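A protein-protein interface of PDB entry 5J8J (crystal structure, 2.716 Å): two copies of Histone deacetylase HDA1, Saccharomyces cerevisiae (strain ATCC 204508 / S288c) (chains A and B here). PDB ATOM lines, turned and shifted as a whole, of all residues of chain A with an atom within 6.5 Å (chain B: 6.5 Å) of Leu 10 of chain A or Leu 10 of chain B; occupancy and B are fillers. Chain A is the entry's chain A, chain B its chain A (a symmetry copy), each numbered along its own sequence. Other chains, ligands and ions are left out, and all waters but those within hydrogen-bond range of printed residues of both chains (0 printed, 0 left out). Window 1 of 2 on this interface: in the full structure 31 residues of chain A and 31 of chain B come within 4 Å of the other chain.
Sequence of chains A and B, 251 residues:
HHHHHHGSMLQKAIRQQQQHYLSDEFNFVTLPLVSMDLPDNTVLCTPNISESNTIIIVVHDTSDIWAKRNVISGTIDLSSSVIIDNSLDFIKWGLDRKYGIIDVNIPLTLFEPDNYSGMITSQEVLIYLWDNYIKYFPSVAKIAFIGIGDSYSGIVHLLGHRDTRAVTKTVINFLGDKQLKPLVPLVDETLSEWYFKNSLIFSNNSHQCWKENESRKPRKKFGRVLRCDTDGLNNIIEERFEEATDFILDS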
ATOM      1  N   HIS A   6     -16.459  13.703   8.249  1.00  0.00           N
ATOM      2  CA  HIS A   6     -15.954  14.122   9.532  1.00  0.00           C
ATOM      3  C   HIS A   6     -15.345  12.890  10.212  1.00  0.00           C
ATOM      4  O   HIS A   6     -14.764  12.977  11.285  1.00  0.00           O
ATOM      5  CB  HIS A   6     -17.104  14.758  10.321  1.00  0.00           C
ATOM      6  CG  HIS A   6     -16.683  15.499  11.542  1.00  0.00           C
ATOM      7  ND1 HIS A   6     -17.265  15.295  12.774  1.00  0.00           N
ATOM      8  CD2 HIS A   6     -15.732  16.449  11.732  1.00  0.00           C
ATOM      9  CE1 HIS A   6     -16.691  16.073  13.669  1.00  0.00           C
ATOM     10  NE2 HIS A   6     -15.757  16.784  13.062  1.00  0.00           N
ATOM     11  N   GLY A   7     -15.432  11.745   9.539  1.00  0.00           N
ATOM     12  CA  GLY A   7     -14.974  10.492  10.106  1.00  0.00           C
ATOM     13  C   GLY A   7     -13.512  10.374  10.491  1.00  0.00           C
ATOM     14  O   GLY A   7     -13.187   9.701  11.455  1.00  0.00           O
ATOM     15  N   SER A   8     -12.610  10.985   9.738  1.00  0.00           N
ATOM     16  CA  SER A   8     -11.188  10.861  10.055  1.00  0.00           C
ATOM     17  C   SER A   8     -10.819  11.716  11.230  1.00  0.00           C
ATOM     18  O   SER A   8     -10.040  11.300  12.087  1.00  0.00           O
ATOM     19  CB  SER A   8     -10.303  11.244   8.874  1.00  0.00           C
ATOM     20  OG  SER A   8     -10.489  10.329   7.826  1.00  0.00           O
ATOM     21  N   MET A   9     -11.360  12.926  11.243  1.00  0.00           N
ATOM     22  CA  MET A   9     -11.152  13.849  12.335  1.00  0.00           C
ATOM     23  C   MET A   9     -11.578  13.170  13.644  1.00  0.00           C
ATOM     24  O   MET A   9     -10.849  13.211  14.641  1.00  0.00           O
ATOM     25  CB  MET A   9     -11.931  15.142  12.079  1.00  0.00           C
ATOM     26  CG  MET A   9     -11.721  16.271  13.079  1.00  0.00           C
ATOM     27  SD  MET A   9     -10.015  16.839  13.288  1.00  0.00           S
ATOM     28  CE  MET A   9      -9.632  17.480  11.660  1.00  0.00           C
ATOM     29  N   LEU A  10     -12.734  12.508  13.611  1.00  0.00           N
ATOM     30  CA  LEU A  10     -13.277  11.833  14.781  1.00  0.00           C
ATOM     31  C   LEU A  10     -12.347  10.762  15.321  1.00  0.00           C
ATOM     32  O   LEU A  10     -12.171  10.645  16.519  1.00  0.00           O
ATOM     33  CB  LEU A  10     -14.632  11.212  14.460  1.00  0.00           C
ATOM     34  CG  LEU A  10     -15.706  12.265  14.237  1.00  0.00           C
ATOM     35  CD1 LEU A  10     -17.070  11.648  14.000  1.00  0.00           C
ATOM     36  CD2 LEU A  10     -15.731  13.242  15.379  1.00  0.00           C
ATOM     37  N   GLN A  11     -11.760   9.972  14.435  1.00  0.00           N
ATOM     38  CA  GLN A  11     -10.839   8.916  14.835  1.00  0.00           C
ATOM     39  C   GLN A  11      -9.663   9.454  15.644  1.00  0.00           C
ATOM     40  O   GLN A  11      -9.156   8.784  16.558  1.00  0.00           O
ATOM     41  CB  GLN A  11     -10.306   8.182  13.608  1.00  0.00           C
ATOM     42  CG  GLN A  11     -11.241   7.158  13.028  1.00  0.00           C
ATOM     43  CD  GLN A  11     -10.549   6.315  11.995  1.00  0.00           C
ATOM     44  OE1 GLN A  11     -10.476   5.100  12.126  1.00  0.00           O
ATOM     45  NE2 GLN A  11     -10.038   6.954  10.951  1.00  0.00           N
ATOM     46  N   LYS A  12      -9.222  10.653  15.290  1.00  0.00           N
ATOM     47  CA  LYS A  12      -8.076  11.261  15.937  1.00  0.00           C
ATOM     48  C   LYS A  12      -8.501  11.939  17.229  1.00  0.00           C
ATOM     49  O   LYS A  12      -7.751  11.952  18.200  1.00  0.00           O
ATOM     50  CB  LYS A  12      -7.389  12.247  14.983  1.00  0.00           C
ATOM     51  CG  LYS A  12      -6.994  11.585  13.666  1.00  0.00           C
ATOM     52  CD  LYS A  12      -5.911  12.339  12.917  1.00  0.00           C
ATOM     53  CE  LYS A  12      -5.772  11.797  11.493  1.00  0.00           C
ATOM     54  NZ  LYS A  12      -4.944  12.668  10.602  1.00  0.00           N
ATOM     55  N   ALA A  13      -9.713  12.486  17.236  1.00  0.00           N
ATOM     56  CA  ALA A  13     -10.279  13.104  18.433  1.00  0.00           C
ATOM     57  C   ALA A  13     -10.503  12.074  19.539  1.00  0.00           C
ATOM     58  O   ALA A  13     -10.299  12.360  20.712  1.00  0.00           O
ATOM     59  CB  ALA A  13     -11.589  13.809  18.104  1.00  0.00           C
ATOM     60  N   ILE A  14     -10.943  10.886  19.151  1.00  0.00           N
ATOM     61  CA  ILE A  14     -11.154   9.795  20.088  1.00  0.00           C
ATOM     62  C   ILE A  14      -9.847   9.356  20.749  1.00  0.00           C
ATOM     63  O   ILE A  14      -9.765   9.306  21.961  1.00  0.00           O
ATOM     64  CB  ILE A  14     -11.796   8.580  19.401  1.00  0.00           C
ATOM     65  CG1 ILE A  14     -13.176   8.939  18.851  1.00  0.00           C
ATOM     66  CG2 ILE A  14     -11.905   7.429  20.373  1.00  0.00           C
ATOM     67  CD1 ILE A  14     -13.805   7.840  18.045  1.00  0.00           C
ATOM     68  N   ARG A  15      -8.825   9.066  19.949  1.00  0.00           N
ATOM     69  CA  ARG A  15      -7.554   8.584  20.461  1.00  0.00           C
ATOM     70  C   ARG A  15      -6.888   9.626  21.341  1.00  0.00           C
ATOM     71  O   ARG A  15      -6.115   9.313  22.248  1.00  0.00           O
ATOM     72  CB  ARG A  15      -6.632   8.192  19.307  1.00  0.00           C
ATOM     73  CG  ARG A  15      -5.321   7.543  19.749  1.00  0.00           C
ATOM     74  CD  ARG A  15      -5.517   6.514  20.865  1.00  0.00           C
ATOM     75  NE  ARG A  15      -4.308   5.734  21.106  1.00  0.00           N
ATOM     76  CZ  ARG A  15      -4.239   4.711  21.957  1.00  0.00           C
ATOM     77  NH1 ARG A  15      -5.310   4.352  22.651  1.00  0.00           N
ATOM     78  NH2 ARG A  15      -3.102   4.037  22.102  1.00  0.00           N
ATOM     79  N   GLN A  17      -8.446  12.047  23.289  1.00  0.00           N
ATOM     80  CA  GLN A  17      -9.064  12.101  24.593  1.00  0.00           C
ATOM     81  C   GLN A  17      -8.654  10.888  25.452  1.00  0.00           C
ATOM     82  O   GLN A  17      -8.485  10.994  26.672  1.00  0.00           O
ATOM     83  CB  GLN A  17     -10.575  12.206  24.445  1.00  0.00           C
ATOM     84  CG  GLN A  17     -11.266  12.237  25.763  1.00  0.00           C
ATOM     85  CD  GLN A  17     -12.691  12.702  25.689  1.00  0.00           C
ATOM     86  OE1 GLN A  17     -13.147  13.213  24.672  1.00  0.00           O
ATOM     87  NE2 GLN A  17     -13.410  12.530  26.781  1.00  0.00           N
ATOM     88  N   THR A  62      -9.884   1.970  16.513  1.00  0.00           N
ATOM     89  CA  THR A  62     -10.442   3.129  17.203  1.00  0.00           C
ATOM     90  C   THR A  62     -11.734   2.704  17.933  1.00  0.00           C
ATOM     91  O   THR A  62     -12.515   1.902  17.427  1.00  0.00           O
ATOM     92  CB  THR A  62     -10.712   4.330  16.230  1.00  0.00           C
ATOM     93  OG1 THR A  62     -11.085   3.823  14.949  1.00  0.00           O
ATOM     94  CG2 THR A  62      -9.456   5.202  16.032  1.00  0.00           C
ATOM     95  N   ILE A  65     -18.124   5.354  19.421  1.00  0.00           N
ATOM     96  CA  ILE A  65     -18.781   6.442  20.108  1.00  0.00           C
ATOM     97  C   ILE A  65     -20.249   6.116  20.141  1.00  0.00           C
ATOM     98  O   ILE A  65     -20.852   5.820  19.113  1.00  0.00           O
ATOM     99  CB  ILE A  65     -18.586   7.789  19.404  1.00  0.00           C
ATOM    100  CG1 ILE A  65     -17.110   8.154  19.341  1.00  0.00           C
ATOM    101  CG2 ILE A  65     -19.379   8.895  20.108  1.00  0.00           C
ATOM    102  CD1 ILE A  65     -16.886   9.425  18.606  1.00  0.00           C
ATOM    103  N   ILE A  76     -26.540  13.979  15.948  1.00  0.00           N
ATOM    104  CA  ILE A  76     -26.041  13.344  17.152  1.00  0.00           C
ATOM    105  C   ILE A  76     -26.083  14.274  18.368  1.00  0.00           C
ATOM    106  O   ILE A  76     -25.580  15.391  18.317  1.00  0.00           O
ATOM    107  CB  ILE A  76     -24.593  12.840  16.904  1.00  0.00           C
ATOM    108  CG1 ILE A  76     -24.608  11.451  16.257  1.00  0.00           C
ATOM    109  CG2 ILE A  76     -23.797  12.791  18.202  1.00  0.00           C
ATOM    110  CD1 ILE A  76     -25.257  11.352  14.885  1.00  0.00           C
ATOM    111  N   LEU A  78     -24.640  15.731  21.176  1.00  0.00           N
ATOM    112  CA  LEU A  78     -23.257  15.861  21.627  1.00  0.00           C
ATOM    113  C   LEU A  78     -23.083  15.625  23.123  1.00  0.00           C
ATOM    114  O   LEU A  78     -22.103  15.016  23.546  1.00  0.00           O
ATOM    115  CB  LEU A  78     -22.717  17.240  21.247  1.00  0.00           C
ATOM    116  CG  LEU A  78     -21.615  17.195  20.191  1.00  0.00           C
ATOM    117  CD1 LEU A  78     -22.117  16.482  18.956  1.00  0.00           C
ATOM    118  CD2 LEU A  78     -21.132  18.598  19.852  1.00  0.00           C
ATOM    119  N   SER A  81     -22.916  12.012  23.973  1.00  0.00           N
ATOM    120  CA  SER A  81     -21.879  11.233  23.311  1.00  0.00           C
ATOM    121  C   SER A  81     -20.824  10.753  24.299  1.00  0.00           C
ATOM    122  O   SER A  81     -20.356  11.518  25.143  1.00  0.00           O
ATOM    123  CB  SER A  81     -21.234  12.051  22.192  1.00  0.00           C
ATOM    124  OG  SER A  81     -20.691  13.251  22.695  1.00  0.00           O
ATOM    125  N   HIS B   6     -17.586  12.662  25.608  1.00  0.00           N
ATOM    126  CA  HIS B   6     -16.760  12.897  24.450  1.00  0.00           C
ATOM    127  C   HIS B   6     -17.261  14.182  23.779  1.00  0.00           C
ATOM    128  O   HIS B   6     -16.682  14.666  22.816  1.00  0.00           O
ATOM    129  CB  HIS B   6     -16.830  11.662  23.545  1.00  0.00           C
ATOM    130  CG  HIS B   6     -15.811  11.628  22.461  1.00  0.00           C
ATOM    131  ND1 HIS B   6     -16.134  11.387  21.143  1.00  0.00           N
ATOM    132  CD2 HIS B   6     -14.466  11.807  22.487  1.00  0.00           C
ATOM    133  CE1 HIS B   6     -15.043  11.428  20.405  1.00  0.00           C
ATOM    134  NE2 HIS B   6     -14.017  11.680  21.198  1.00  0.00           N
ATOM    135  N   GLY B   7     -18.314  14.767  24.345  1.00  0.00           N
ATOM    136  CA  GLY B   7     -18.940  15.938  23.763  1.00  0.00           C
ATOM    137  C   GLY B   7     -18.098  17.188  23.595  1.00  0.00           C
ATOM    138  O   GLY B   7     -18.287  17.927  22.644  1.00  0.00           O
ATOM    139  N   SER B   8     -17.190  17.466  24.518  1.00  0.00           N
ATOM    140  CA  SER B   8     -16.388  18.684  24.412  1.00  0.00           C
ATOM    141  C   SER B   8     -15.317  18.536  23.373  1.00  0.00           C
ATOM    142  O   SER B   8     -15.048  19.468  22.615  1.00  0.00           O
ATOM    143  CB  SER B   8     -15.735  19.057  25.738  1.00  0.00           C
ATOM    144  OG  SER B   8     -16.724  19.394  26.675  1.00  0.00           O
ATOM    145  N   MET B   9     -14.688  17.369  23.368  1.00  0.00           N
ATOM    146  CA  MET B   9     -13.673  17.047  22.391  1.00  0.00           C
ATOM    147  C   MET B   9     -14.265  17.227  20.987  1.00  0.00           C
ATOM    148  O   MET B   9     -13.645  17.848  20.117  1.00  0.00           O
ATOM    149  CB  MET B   9     -13.162  15.623  22.622  1.00  0.00           C
ATOM    150  CG  MET B   9     -11.998  15.169  21.752  1.00  0.00           C
ATOM    151  SD  MET B   9     -10.498  16.177  21.846  1.00  0.00           S
ATOM    152  CE  MET B   9     -10.010  15.965  23.556  1.00  0.00           C
ATOM    153  N   LEU B  10     -15.483  16.721  20.795  1.00  0.00           N
ATOM    154  CA  LEU B  10     -16.162  16.795  19.509  1.00  0.00           C
ATOM    155  C   LEU B  10     -16.366  18.224  19.038  1.00  0.00           C
ATOM    156  O   LEU B  10     -16.172  18.523  17.876  1.00  0.00           O
ATOM    157  CB  LEU B  10     -17.511  16.087  19.576  1.00  0.00           C
ATOM    158  CG  LEU B  10     -17.361  14.581  19.712  1.00  0.00           C
ATOM    159  CD1 LEU B  10     -18.699  13.870  19.693  1.00  0.00           C
ATOM    160  CD2 LEU B  10     -16.435  14.046  18.654  1.00  0.00           C
ATOM    161  N   GLN B  11     -16.769  19.104  19.942  1.00  0.00           N
ATOM    162  CA  GLN B  11     -16.987  20.506  19.608  1.00  0.00           C
ATOM    163  C   GLN B  11     -15.736  21.161  19.028  1.00  0.00           C
ATOM    164  O   GLN B  11     -15.821  22.037  18.154  1.00  0.00           O
ATOM    165  CB  GLN B  11     -17.429  21.285  20.844  1.00  0.00           C
ATOM    166  CG  GLN B  11     -18.882  21.135  21.198  1.00  0.00           C
ATOM    167  CD  GLN B  11     -19.286  22.119  22.259  1.00  0.00           C
ATOM    168  OE1 GLN B  11     -20.177  22.931  22.050  1.00  0.00           O
ATOM    169  NE2 GLN B  11     -18.635  22.051  23.413  1.00  0.00           N
ATOM    170  N   LYS B  12     -14.583  20.745  19.532  1.00  0.00           N
ATOM    171  CA  LYS B  12     -13.320  21.321  19.113  1.00  0.00           C
ATOM    172  C   LYS B  12     -12.847  20.666  17.826  1.00  0.00           C
ATOM    173  O   LYS B  12     -12.241  21.320  16.983  1.00  0.00           O
ATOM    174  CB  LYS B  12     -12.278  21.185  20.231  1.00  0.00           C
ATOM    175  CG  LYS B  12     -12.760  21.804  21.539  1.00  0.00           C
ATOM    176  CD  LYS B  12     -11.631  22.138  22.497  1.00  0.00           C
ATOM    177  CE  LYS B  12     -12.189  22.474  23.881  1.00  0.00           C
ATOM    178  NZ  LYS B  12     -11.143  22.524  24.950  1.00  0.00           N
ATOM    179  N   ALA B  13     -13.143  19.379  17.676  1.00  0.00           N
ATOM    180  CA  ALA B  13     -12.815  18.643  16.457  1.00  0.00           C
ATOM    181  C   ALA B  13     -13.592  19.181  15.257  1.00  0.00           C
ATOM    182  O   ALA B  13     -13.068  19.253  14.152  1.00  0.00           O
ATOM    183  CB  ALA B  13     -13.096  17.156  16.636  1.00  0.00           C
ATOM    184  N   ILE B  14     -14.849  19.535  15.484  1.00  0.00           N
ATOM    185  CA  ILE B  14     -15.691  20.109  14.448  1.00  0.00           C
ATOM    186  C   ILE B  14     -15.153  21.455  13.961  1.00  0.00           C
ATOM    187  O   ILE B  14     -14.960  21.640  12.774  1.00  0.00           O
ATOM    188  CB  ILE B  14     -17.135  20.298  14.938  1.00  0.00           C
ATOM    189  CG1 ILE B  14     -17.762  18.953  15.298  1.00  0.00           C
ATOM    190  CG2 ILE B  14     -17.958  20.992  13.877  1.00  0.00           C
ATOM    191  CD1 ILE B  14     -19.125  19.072  15.916  1.00  0.00           C
ATOM    192  N   ARG B  15     -14.889  22.376  14.882  1.00  0.00           N
ATOM    193  CA  ARG B  15     -14.429  23.710  14.533  1.00  0.00           C
ATOM    194  C   ARG B  15     -13.078  23.659  13.845  1.00  0.00           C
ATOM    195  O   ARG B  15     -12.724  24.526  13.044  1.00  0.00           O
ATOM    196  CB  ARG B  15     -14.358  24.589  15.781  1.00  0.00           C
ATOM    197  CG  ARG B  15     -14.017  26.051  15.496  1.00  0.00           C
ATOM    198  CD  ARG B  15     -14.774  26.611  14.290  1.00  0.00           C
ATOM    199  NE  ARG B  15     -14.626  28.058  14.176  1.00  0.00           N
ATOM    200  CZ  ARG B  15     -15.260  28.803  13.273  1.00  0.00           C
ATOM    201  NH1 ARG B  15     -16.080  28.233  12.399  1.00  0.00           N
ATOM    202  NH2 ARG B  15     -15.087  30.121  13.251  1.00  0.00           N
ATOM    203  N   GLN B  17     -11.815  21.093  11.869  1.00  0.00           N
ATOM    204  CA  GLN B  17     -11.945  20.671  10.493  1.00  0.00           C
ATOM    205  C   GLN B  17     -12.524  21.801   9.618  1.00  0.00           C
ATOM    206  O   GLN B  17     -12.155  21.960   8.449  1.00  0.00           O
ATOM    207  CB  GLN B  17     -12.790  19.407  10.419  1.00  0.00           C
ATOM    208  CG  GLN B  17     -12.981  18.943   9.018  1.00  0.00           C
ATOM    209  CD  GLN B  17     -13.481  17.532   8.910  1.00  0.00           C
ATOM    210  OE1 GLN B  17     -13.507  16.785   9.882  1.00  0.00           O
ATOM    211  NE2 GLN B  17     -13.883  17.153   7.712  1.00  0.00           N
ATOM    212  N   THR B  62     -21.621  25.644  17.583  1.00  0.00           N
ATOM    213  CA  THR B  62     -20.940  24.545  16.905  1.00  0.00           C
ATOM    214  C   THR B  62     -21.938  23.844  15.958  1.00  0.00           C
ATOM    215  O   THR B  62     -23.113  23.685  16.279  1.00  0.00           O
ATOM    216  CB  THR B  62     -20.305  23.523  17.912  1.00  0.00           C
ATOM    217  OG1 THR B  62     -21.120  23.446  19.081  1.00  0.00           O
ATOM    218  CG2 THR B  62     -18.896  23.961  18.361  1.00  0.00           C
ATOM    219  N   ILE B  65     -23.461  17.305  13.724  1.00  0.00           N
ATOM    220  CA  ILE B  65     -22.895  16.172  13.028  1.00  0.00           C
ATOM    221  C   ILE B  65     -24.026  15.221  12.750  1.00  0.00           C
ATOM    222  O   ILE B  65     -24.775  14.852  13.650  1.00  0.00           O
ATOM    223  CB  ILE B  65     -21.826  15.446  13.851  1.00  0.00           C
ATOM    224  CG1 ILE B  65     -20.664  16.378  14.163  1.00  0.00           C
ATOM    225  CG2 ILE B  65     -21.326  14.197  13.119  1.00  0.00           C
ATOM    226  CD1 ILE B  65     -19.641  15.720  15.015  1.00  0.00           C
ATOM    227  N   ILE B  76     -22.249   5.139  16.516  1.00  0.00           N
ATOM    228  CA  ILE B  76     -22.267   6.010  15.358  1.00  0.00           C
ATOM    229  C   ILE B  76     -21.377   5.497  14.222  1.00  0.00           C
ATOM    230  O   ILE B  76     -20.206   5.202  14.430  1.00  0.00           O
ATOM    231  CB  ILE B  76     -21.833   7.439  15.783  1.00  0.00           C
ATOM    232  CG1 ILE B  76     -23.031   8.232  16.316  1.00  0.00           C
ATOM    233  CG2 ILE B  76     -21.198   8.192  14.620  1.00  0.00           C
ATOM    234  CD1 ILE B  76     -23.705   7.680  17.562  1.00  0.00           C
ATOM    235  N   LEU B  78     -18.943   5.946  11.779  1.00  0.00           N
ATOM    236  CA  LEU B  78     -17.945   6.986  11.554  1.00  0.00           C
ATOM    237  C   LEU B  78     -17.799   7.379  10.087  1.00  0.00           C
ATOM    238  O   LEU B  78     -17.627   8.555   9.774  1.00  0.00           O
ATOM    239  CB  LEU B  78     -16.594   6.536  12.112  1.00  0.00           C
ATOM    240  CG  LEU B  78     -16.128   7.352  13.316  1.00  0.00           C
ATOM    241  CD1 LEU B  78     -17.176   7.303  14.404  1.00  0.00           C
ATOM    242  CD2 LEU B  78     -14.787   6.846  13.827  1.00  0.00           C
ATOM    243  N   SER B  81     -20.411   9.790   9.007  1.00  0.00           N
ATOM    244  CA  SER B  81     -20.502  11.034   9.759  1.00  0.00           C
ATOM    245  C   SER B  81     -20.098  12.232   8.908  1.00  0.00           C
ATOM    246  O   SER B  81     -19.088  12.193   8.203  1.00  0.00           O
ATOM    247  CB  SER B  81     -19.641  10.957  11.020  1.00  0.00           C
ATOM    248  OG  SER B  81     -18.297  10.685  10.695  1.00  0.00           O
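The backbone carbonyl oxygen (O) of Ser 81 of chain B is in hydrogen-bond range of the backbone NH (N) of His 6 of chain A, at 3.0 Å.
The backbone NH (N) of Gly 7 of chain A sits at hydrogen-bond distance from the side-chain hydroxyl (OG) of Ser 81 of chain B.
The backbone carbonyl oxygen of Ile 65 of chain A is in hydrogen-bond range of the backbone NH of Ile 76 of chain B (3.0 Å).
The backbone NH (N) of Ile 76 of chain A is in hydrogen-bond range of the backbone carbonyl oxygen (O) of Ile 65 of chain B.
The backbone carbonyl oxygen (O) of Ser 81 of chain A is in hydrogen-bond range of the backbone NH (N) of His 6 of chain B (3.0 Å).
The backbone NH of Gly 7 of chain B sits at hydrogen-bond distance from the side-chain hydroxyl of Ser 81 of chain A (3.3 Å).
The side-chain hydroxyl (OG1) of Thr 62 of chain A sits at hydrogen-bond distance from the side-chain amide oxygen (OE1) of Gln 11 of chain A.
The backbone carbonyl oxygen of Leu 78 of chain A is in hydrogen-bond range of the side-chain hydroxyl of Ser 81 of chain A.
The side-chain amide oxygen (OE1) of Gln 11 of chain B is in hydrogen-bond range of the side-chain hydroxyl (OG1) of Thr 62 of chain B, 3.2 Å away.
OG of Ser 81 of chain B sits at hydrogen-bond distance from O of Leu 78 of chain B, 2.4 Å away.
His 6 of chain A touches Ala 13 of chain B.
CD1 of Ile 65 of chain B touches CE1 of His 6 of chain A, 3.3 Å away.
Ala 13 of chain B touches Met 9 of chain A (O to CG, 3.4 Å).
Leu 10 of chain B touches Leu 10 of chain A.
Leu 10 of chain A touches Ser 81 of chain B.
Gln 11 of chain A touches Leu 78 of chain B.
His 6 of chain B touches Ala 13 of chain A.
CG1 of Ile 14 of chain A touches CE1 of His 6 of chain B, at 3.5 Å.
CG1 of Ile 76 of chain B touches CG1 of Ile 76 of chain A, 3.6 Å away.
CD2 of Leu 78 of chain A touches CG of Gln 11 of chain B, 3.6 Å away.
Leu 10 of chain A touches just these residues of chain B: Leu 10 (3.4 Å) and Ser 81 (3.7 Å).
Leu 10 of chain B touches two residues of chain A.
Of the printed residues of chain A, Ile 14 of chain B touches His 6.
Of the printed residues of chain A, Ile 65 of chain B touches His 6 and Ile 76.
Of the printed residues of chain A, Gln 11 of chain B touches Leu 78 (3.6 Å).
The nearest residue of chain B that does not touch Leu 10 of chain A is Leu 78 of chain B (4.3 Å).
The nearest residue of chain A that does not touch Leu 10 of chain B is Leu 78 of chain A (4.3 Å).
Hydrophobic or aromatic side chains of chain A that line the printed part of chain B: His 6, Met 9, Leu 10, Ala 13, Ile 14, Ile 65, Ile 76 and Leu 78.
Hydrophobic or aromatic side chains of chain B that line the printed part of chain A: His 6, Met 9, Leu 10, Ala 13, Ile 14, Ile 65, Ile 76 and Leu 78.
Among the printed residues, no Asp or Glu carboxylate lies within 4 Å of a Lys or Arg side-chain nitrogen of the other chain.
His 6 of chain A touches Ala 13 of chain B, and with the chains exchanged Ala 13 of chain A touches His 6 of chain B.
Gly 7 of chain A touches Leu 78 of chain B, and with the chains exchanged Leu 78 of chain A touches Gly 7 of chain B.
Met 9 of chain A touches Gln 17 of chain B, and with the chains exchanged Gln 17 of chain A touches Met 9 of chain B.
Ile 76 of chain B touches its own counterpart, Ile 76 of chain A.
16 positions are printed for both chains.
Of the 27 pairs that touch across the chains among the printed residues, 27 have their exchanged pair printed and touching as well.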
